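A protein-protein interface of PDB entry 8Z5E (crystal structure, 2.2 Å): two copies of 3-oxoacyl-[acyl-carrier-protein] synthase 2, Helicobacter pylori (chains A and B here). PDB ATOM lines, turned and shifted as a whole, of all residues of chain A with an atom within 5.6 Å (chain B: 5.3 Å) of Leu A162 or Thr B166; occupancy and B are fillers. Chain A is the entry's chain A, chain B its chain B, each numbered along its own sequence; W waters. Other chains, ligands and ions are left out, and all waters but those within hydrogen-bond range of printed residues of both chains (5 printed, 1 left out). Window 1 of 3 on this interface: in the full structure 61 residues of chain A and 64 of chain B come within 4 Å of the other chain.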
ATOM      1  N   VAL A 107      17.220 -26.881  33.194  1.00  0.00           N
ATOM      2  CA  VAL A 107      16.712 -26.419  31.911  1.00  0.00           C
ATOM      3  C   VAL A 107      17.622 -26.957  30.813  1.00  0.00           C
ATOM      4  O   VAL A 107      18.856 -26.902  30.920  1.00  0.00           O
ATOM      5  CB  VAL A 107      16.576 -24.879  31.856  1.00  0.00           C
ATOM      6  CG1 VAL A 107      17.885 -24.175  32.203  1.00  0.00           C
ATOM      7  CG2 VAL A 107      16.027 -24.399  30.498  1.00  0.00           C
ATOM      8  N   SER A 108      17.011 -27.560  29.803  1.00  0.00           N
ATOM      9  CA  SER A 108      17.715 -28.056  28.629  1.00  0.00           C
ATOM     10  C   SER A 108      17.184 -27.285  27.432  1.00  0.00           C
ATOM     11  O   SER A 108      15.990 -27.371  27.119  1.00  0.00           O
ATOM     12  CB  SER A 108      17.498 -29.556  28.444  1.00  0.00           C
ATOM     13  OG  SER A 108      18.231 -30.027  27.327  1.00  0.00           O
ATOM     14  N   SER A 109      18.041 -26.502  26.797  1.00  0.00           N
ATOM     15  CA  SER A 109      17.601 -25.673  25.686  1.00  0.00           C
ATOM     16  C   SER A 109      18.264 -26.122  24.390  1.00  0.00           C
ATOM     17  O   SER A 109      19.330 -26.752  24.393  1.00  0.00           O
ATOM     18  CB  SER A 109      17.884 -24.196  25.970  1.00  0.00           C
ATOM     19  OG  SER A 109      19.279 -23.945  26.036  1.00  0.00           O
ATOM     20  N   ASN A 145      22.797 -20.564  24.384  1.00  0.00           N
ATOM     21  CA  ASN A 145      22.510 -20.979  25.753  1.00  0.00           C
ATOM     22  C   ASN A 145      21.831 -19.889  26.557  1.00  0.00           C
ATOM     23  O   ASN A 145      21.399 -20.152  27.684  1.00  0.00           O
ATOM     24  CB  ASN A 145      23.791 -21.437  26.457  1.00  0.00           C
ATOM     25  CG  ASN A 145      24.721 -20.275  26.795  1.00  0.00           C
ATOM     26  OD1 ASN A 145      25.187 -19.563  25.911  1.00  0.00           O
ATOM     27  ND2 ASN A 145      24.977 -20.076  28.075  1.00  0.00           N
ATOM     28  N   PRO A 160      20.740 -28.406  36.539  1.00  0.00           N
ATOM     29  CA  PRO A 160      21.630 -28.406  35.368  1.00  0.00           C
ATOM     30  C   PRO A 160      21.076 -27.545  34.241  1.00  0.00           C
ATOM     31  O   PRO A 160      19.886 -27.595  33.922  1.00  0.00           O
ATOM     32  CB  PRO A 160      21.698 -29.891  34.983  1.00  0.00           C
ATOM     33  CG  PRO A 160      21.564 -30.602  36.306  1.00  0.00           C
ATOM     34  CD  PRO A 160      20.493 -29.770  37.033  1.00  0.00           C
ATOM     35  N   ASN A 161      21.942 -26.718  33.674  1.00  0.00           N
ATOM     36  CA  ASN A 161      21.570 -25.687  32.701  1.00  0.00           C
ATOM     37  C   ASN A 161      22.367 -26.014  31.449  1.00  0.00           C
ATOM     38  O   ASN A 161      23.560 -25.698  31.362  1.00  0.00           O
ATOM     39  CB  ASN A 161      21.875 -24.292  33.242  1.00  0.00           C
ATOM     40  CG  ASN A 161      21.173 -23.188  32.488  1.00  0.00           C
ATOM     41  OD1 ASN A 161      21.369 -23.001  31.285  1.00  0.00           O
ATOM     42  ND2 ASN A 161      20.372 -22.414  33.209  1.00  0.00           N
ATOM     43  N   LEU A 162      21.709 -26.695  30.508  1.00  0.00           N
ATOM     44  CA  LEU A 162      22.377 -27.367  29.402  1.00  0.00           C
ATOM     45  C   LEU A 162      21.767 -26.909  28.088  1.00  0.00           C
ATOM     46  O   LEU A 162      20.592 -26.539  28.033  1.00  0.00           O
ATOM     47  CB  LEU A 162      22.265 -28.888  29.543  1.00  0.00           C
ATOM     48  CG  LEU A 162      22.443 -29.445  30.969  1.00  0.00           C
ATOM     49  CD1 LEU A 162      21.957 -30.887  31.073  1.00  0.00           C
ATOM     50  CD2 LEU A 162      23.901 -29.347  31.425  1.00  0.00           C
ATOM     51  N   SER A 163      22.567 -26.951  27.024  1.00  0.00           N
ATOM     52  CA  SER A 163      22.106 -26.439  25.742  1.00  0.00           C
ATOM     53  C   SER A 163      22.684 -27.257  24.598  1.00  0.00           C
ATOM     54  O   SER A 163      23.890 -27.517  24.568  1.00  0.00           O
ATOM     55  CB  SER A 163      22.480 -24.961  25.583  1.00  0.00           C
ATOM     56  OG  SER A 163      21.502 -24.287  24.813  1.00  0.00           O
ATOM     57  N   SER A 164      21.817 -27.628  23.653  1.00  0.00           N
ATOM     58  CA  SER A 164      22.155 -28.451  22.498  1.00  0.00           C
ATOM     59  C   SER A 164      22.132 -27.593  21.233  1.00  0.00           C
ATOM     60  O   SER A 164      21.215 -26.782  21.033  1.00  0.00           O
ATOM     61  CB  SER A 164      21.173 -29.633  22.345  1.00  0.00           C
ATOM     62  OG  SER A 164      21.061 -30.419  23.544  1.00  0.00           O
ATOM     63  N   GLU A 177      18.817 -34.846  26.253  1.00  0.00           N
ATOM     64  CA  GLU A 177      19.770 -34.495  27.304  1.00  0.00           C
ATOM     65  C   GLU A 177      19.053 -34.300  28.631  1.00  0.00           C
ATOM     66  O   GLU A 177      19.546 -34.731  29.681  1.00  0.00           O
ATOM     67  CB  GLU A 177      20.556 -33.223  26.938  1.00  0.00           C
ATOM     68  CG  GLU A 177      21.856 -33.123  27.727  1.00  0.00           C
ATOM     69  CD  GLU A 177      22.801 -32.007  27.285  1.00  0.00           C
ATOM     70  OE1 GLU A 177      22.461 -31.189  26.396  1.00  0.00           O
ATOM     71  OE2 GLU A 177      23.934 -31.988  27.812  1.00  0.00           O
ATOM     72  N   ALA A 178      17.876 -33.673  28.595  1.00  0.00           N
ATOM     73  CA  ALA A 178      17.059 -33.564  29.800  1.00  0.00           C
ATOM     74  C   ALA A 178      16.662 -34.937  30.331  1.00  0.00           C
ATOM     75  O   ALA A 178      16.694 -35.177  31.543  1.00  0.00           O
ATOM     76  CB  ALA A 178      15.814 -32.741  29.504  1.00  0.00           C
ATOM     77  N   THR A 181      19.727 -36.549  31.929  1.00  0.00           N
ATOM     78  CA  THR A 181      20.012 -35.893  33.202  1.00  0.00           C
ATOM     79  C   THR A 181      19.118 -36.432  34.322  1.00  0.00           C
ATOM     80  O   THR A 181      19.595 -36.743  35.423  1.00  0.00           O
ATOM     81  CB  THR A 181      19.844 -34.375  33.038  1.00  0.00           C
ATOM     82  OG1 THR A 181      20.738 -33.907  32.020  1.00  0.00           O
ATOM     83  CG2 THR A 181      20.189 -33.642  34.331  1.00  0.00           C
ATOM     84  N   MET A 190      12.940 -31.110  34.542  1.00  0.00           N
ATOM     85  CA  MET A 190      13.675 -30.299  33.578  1.00  0.00           C
ATOM     86  C   MET A 190      12.685 -29.570  32.692  1.00  0.00           C
ATOM     87  O   MET A 190      11.698 -30.154  32.232  1.00  0.00           O
ATOM     88  CB  MET A 190      14.658 -31.141  32.734  1.00  0.00           C
ATOM     89  CG  MET A 190      15.700 -31.788  33.639  1.00  0.00           C
ATOM     90  SD  MET A 190      17.125 -30.714  33.964  1.00  0.00           S
ATOM     91  CE  MET A 190      17.478 -30.000  32.366  1.00  0.00           C
ATOM     92  N   SER B 111      31.475 -25.620  21.782  1.00  0.00           N
ATOM     93  CA  SER B 111      31.939 -24.288  21.422  1.00  0.00           C
ATOM     94  C   SER B 111      30.901 -23.295  21.928  1.00  0.00           C
ATOM     95  O   SER B 111      29.711 -23.625  22.028  1.00  0.00           O
ATOM     96  CB  SER B 111      32.128 -24.140  19.902  1.00  0.00           C
ATOM     97  OG  SER B 111      32.800 -22.931  19.567  1.00  0.00           O
ATOM     98  N   SER B 164      27.454 -29.243  22.797  1.00  0.00           N
ATOM     99  CA  SER B 164      27.135 -28.339  23.897  1.00  0.00           C
ATOM    100  C   SER B 164      27.506 -26.909  23.522  1.00  0.00           C
ATOM    101  O   SER B 164      28.525 -26.678  22.874  1.00  0.00           O
ATOM    102  CB  SER B 164      27.884 -28.764  25.156  1.00  0.00           C
ATOM    103  OG  SER B 164      27.646 -30.140  25.455  1.00  0.00           O
ATOM    104  N   VAL B 165      26.680 -25.944  23.923  1.00  0.00           N
ATOM    105  CA  VAL B 165      26.941 -24.557  23.526  1.00  0.00           C
ATOM    106  C   VAL B 165      26.704 -23.639  24.720  1.00  0.00           C
ATOM    107  O   VAL B 165      26.248 -22.498  24.574  1.00  0.00           O
ATOM    108  CB  VAL B 165      26.093 -24.173  22.295  1.00  0.00           C
ATOM    109  CG1 VAL B 165      24.605 -24.127  22.639  1.00  0.00           C
ATOM    110  CG2 VAL B 165      26.576 -22.873  21.627  1.00  0.00           C
ATOM    111  N   THR B 166      27.031 -24.131  25.914  1.00  0.00           N
ATOM    112  CA  THR B 166      26.847 -23.374  27.148  1.00  0.00           C
ATOM    113  C   THR B 166      28.018 -22.413  27.397  1.00  0.00           C
ATOM    114  O   THR B 166      28.717 -22.486  28.405  1.00  0.00           O
ATOM    115  CB  THR B 166      26.657 -24.326  28.325  1.00  0.00           C
ATOM    116  OG1 THR B 166      27.471 -25.492  28.143  1.00  0.00           O
ATOM    117  CG2 THR B 166      25.197 -24.731  28.459  1.00  0.00           C
ATOM    118  N   ALA B 167      28.202 -21.489  26.455  1.00  0.00           N
ATOM    119  CA  ALA B 167      29.119 -20.359  26.595  1.00  0.00           C
ATOM    120  C   ALA B 167      30.508 -20.812  27.065  1.00  0.00           C
ATOM    121  O   ALA B 167      31.052 -21.772  26.510  1.00  0.00           O
ATOM    122  CB  ALA B 167      28.518 -19.305  27.536  1.00  0.00           C
ATOM    123  N   CYS B 168      31.077 -20.173  28.083  1.00  0.00           N
ATOM    124  CA  CYS B 168      32.470 -20.486  28.532  1.00  0.00           C
ATOM    125  C   CYS B 168      32.527 -21.807  29.321  1.00  0.00           C
ATOM    126  O   CYS B 168      33.630 -22.198  29.722  1.00  0.00           O
ATOM    127  CB  CYS B 168      33.090 -19.311  29.303  1.00  0.00           C
ATOM    128  SG  CYS B 168      33.285 -17.761  28.402  1.00  0.00           S
ATOM    129  N   ALA B 169      31.397 -22.488  29.509  1.00  0.00           N
ATOM    130  CA  ALA B 169      31.472 -23.811  30.122  1.00  0.00           C
ATOM    131  C   ALA B 169      31.253 -24.943  29.100  1.00  0.00           C
ATOM    132  O   ALA B 169      31.169 -26.118  29.471  1.00  0.00           O
ATOM    133  CB  ALA B 169      30.471 -23.916  31.251  1.00  0.00           C
ATOM    134  N   ALA B 170      31.189 -24.587  27.814  1.00  0.00           N
ATOM    135  CA  ALA B 170      30.848 -25.571  26.783  1.00  0.00           C
ATOM    136  C   ALA B 170      31.816 -26.748  26.765  1.00  0.00           C
ATOM    137  O   ALA B 170      31.399 -27.900  26.583  1.00  0.00           O
ATOM    138  CB  ALA B 170      30.807 -24.895  25.407  1.00  0.00           C
ATOM    139  N   HIS B 173      31.014 -29.080  29.681  1.00  0.00           N
ATOM    140  CA  HIS B 173      29.755 -29.771  29.468  1.00  0.00           C
ATOM    141  C   HIS B 173      29.868 -30.813  28.359  1.00  0.00           C
ATOM    142  O   HIS B 173      29.221 -31.857  28.434  1.00  0.00           O
ATOM    143  CB  HIS B 173      28.665 -28.756  29.161  1.00  0.00           C
ATOM    144  CG  HIS B 173      28.157 -28.052  30.376  1.00  0.00           C
ATOM    145  ND1 HIS B 173      27.913 -26.697  30.404  1.00  0.00           N
ATOM    146  CD2 HIS B 173      27.860 -28.514  31.612  1.00  0.00           C
ATOM    147  CE1 HIS B 173      27.461 -26.359  31.598  1.00  0.00           C
ATOM    148  NE2 HIS B 173      27.415 -27.443  32.350  1.00  0.00           N
ATOM    149  N   LYS B 180      27.739 -38.985  30.452  1.00  0.00           N
ATOM    150  CA  LYS B 180      26.352 -39.425  30.576  1.00  0.00           C
ATOM    151  C   LYS B 180      25.994 -40.461  29.514  1.00  0.00           C
ATOM    152  O   LYS B 180      25.320 -41.452  29.805  1.00  0.00           O
ATOM    153  CB  LYS B 180      25.404 -38.229  30.466  1.00  0.00           C
ATOM    154  CG  LYS B 180      25.418 -37.281  31.654  1.00  0.00           C
ATOM    155  CD  LYS B 180      24.273 -36.277  31.516  1.00  0.00           C
ATOM    156  CE  LYS B 180      24.267 -35.245  32.641  1.00  0.00           C
ATOM    157  NZ  LYS B 180      23.716 -33.961  32.118  1.00  0.00           N
ATOM    158  N   GLU B 267      26.772 -30.161  37.663  1.00  0.00           N
ATOM    159  CA  GLU B 267      26.224 -29.117  36.819  1.00  0.00           C
ATOM    160  C   GLU B 267      25.135 -28.378  37.581  1.00  0.00           C
ATOM    161  O   GLU B 267      24.325 -28.995  38.285  1.00  0.00           O
ATOM    162  CB  GLU B 267      25.645 -29.673  35.503  1.00  0.00           C
ATOM    163  CG  GLU B 267      26.274 -30.962  35.004  1.00  0.00           C
ATOM    164  CD  GLU B 267      25.494 -31.620  33.854  1.00  0.00           C
ATOM    165  OE1 GLU B 267      24.494 -32.336  34.134  1.00  0.00           O
ATOM    166  OE2 GLU B 267      25.901 -31.439  32.675  1.00  0.00           O
ATOM    167  N   GLY B 400      29.761 -20.219  32.658  1.00  0.00           N
ATOM    168  CA  GLY B 400      29.462 -19.500  31.408  1.00  0.00           C
ATOM    169  C   GLY B 400      28.371 -18.458  31.563  1.00  0.00           C
ATOM    170  O   GLY B 400      27.645 -18.511  32.572  1.00  0.00           O
ATOM    171  N   THR B 404      25.657 -20.704  33.891  1.00  0.00           N
ATOM    172  CA  THR B 404      25.728 -22.155  33.781  1.00  0.00           C
ATOM    173  C   THR B 404      27.102 -22.668  34.214  1.00  0.00           C
ATOM    174  O   THR B 404      28.137 -22.183  33.742  1.00  0.00           O
ATOM    175  CB  THR B 404      25.406 -22.610  32.353  1.00  0.00           C
ATOM    176  OG1 THR B 404      25.434 -24.043  32.285  1.00  0.00           O
ATOM    177  CG2 THR B 404      26.392 -22.019  31.344  1.00  0.00           C
HETATM  178  O   HOH W   1      24.707 -26.469  34.084  1.00  0.00           O
HETATM  179  O   HOH W   2      25.526 -27.641  27.371  1.00  0.00           O
HETATM  180  O   HOH W   3      24.250 -30.581  24.803  1.00  0.00           O
HETATM  181  O   HOH W   4      25.734 -30.352  27.536  1.00  0.00           O
HETATM  182  O   HOH W   5      27.342 -19.714  24.171  1.00  0.00           O
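OD1 of Asn A145 sits close to O of Val B165, at 3.4 Å. O of Ser A163 is in hydrogen-bond range of N of Val B165 (3.3 Å). O of Asn A161 lies within hydrogen-bond range of OG1 of Thr B404, 2.7 Å away. The side-chain hydroxyl (OG1) of Thr A181 lies within hydrogen-bond range of the side-chain amino group (NZ) of Lys B180.
Printed residues of chain A that touch a printed residue of chain B: Asn A145, Pro A160, Asn A161, Leu A162, Ser A163 and Thr A181. Hydrophobic or aromatic side chains of chain A within 4 Å of the printed part of chain B: Pro A160 and Leu A162. Of the 13 printed residues of chain B, 8 touch a printed residue of chain A.
Among the printed residues, pairs that only touch across the chains: Leu A162 with Glu B267 (3.2 Å), Ser A163 with Ser B164 (3.4 Å), Asn A161 with Thr B166 (3.5 Å), Asn A145 with Ala B167 (3.6 Å), Asn A145 with Thr B166 (3.7 Å), Leu A162 with Lys B180 (3.7 Å), Ser A163 with Thr B166 (3.7 Å), Pro A160 with Glu B267 (3.8 Å), Asn A161 with His B173 (3.96 Å) and Leu A162 with Thr B166 (3.97 Å).
O of Val A107 lies within hydrogen-bond range of N of Leu A162, at 2.9 Å. The backbone NH (N) of Ser A109 is in hydrogen-bond range of the backbone carbonyl oxygen (O) of Leu A162 (2.8 Å). OG of Ser A109 lies within hydrogen-bond range of OG of Ser A163, 2.6 Å away. The backbone NH (N) of Val A107 is in hydrogen-bond range of the backbone carbonyl oxygen (O) of Pro A160. N of Ser B111 is in hydrogen-bond range of O of Ser B164 (3.3 Å). O of Glu A177 is in hydrogen-bond range of OG1 of Thr A181 (2.8 Å).
1 position is printed for both chains. Of the 14 pairs that touch across the chains among the printed residues, none has its exchanged pair printed and touching as well.
Water W4 bridges the side-chain carboxylate of Glu A177 (2.4 Å) and the side-chain hydroxyl of Ser B164 (2.8 Å). Water W3 lies within hydrogen-bond range of OE1 of Glu A177 (2.5 Å), O of Ser A163 (3.1 Å), OG of Ser A164 (3.4 Å) and OG of Ser B164 (3.5 Å). Water W5 lies within hydrogen-bond range of OD1 of Asn A145 (2.8 Å), N of Ala B167 (3.0 Å) and O of Val B165 (3.0 Å). Water W1 lies within hydrogen-bond range of N of Asn A161 (2.8 Å), OG1 of Thr B404 (3.1 Å) and NE2 of His B173 (3.4 Å). Water W2 lies within hydrogen-bond range of the side-chain hydroxyl of Thr B166 (3.0 Å) and the backbone NH of Ser A163 (3.1 Å).
Of the printed residues of chain B, Leu A162 touches Thr B166 (3.97 Å), Lys B180 (3.7 Å) and Glu B267 (3.2 Å). Thr B166 touches just these residues of chain A: Asn A145, Asn A161, Leu A162 and Ser A163. Printed residues of chain A within 4 Å of Ser B164: Ser A163 (3.4 Å). Of the printed residues of chain B, Pro A160 touches Glu B267. Printed residues of chain A within 4 Å of Val B165: Asn A145 and Ser A163. Of the printed residues of chain B, Asn A161 touches Thr B166, His B173 and Thr B404. Ala B170 touches none of the printed residues of chain A. Cys B168 touches none of the printed residues of chain A. The nearest printed residue of chain A that does not touch Thr B166 is Ser A109 (6.4 Å).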
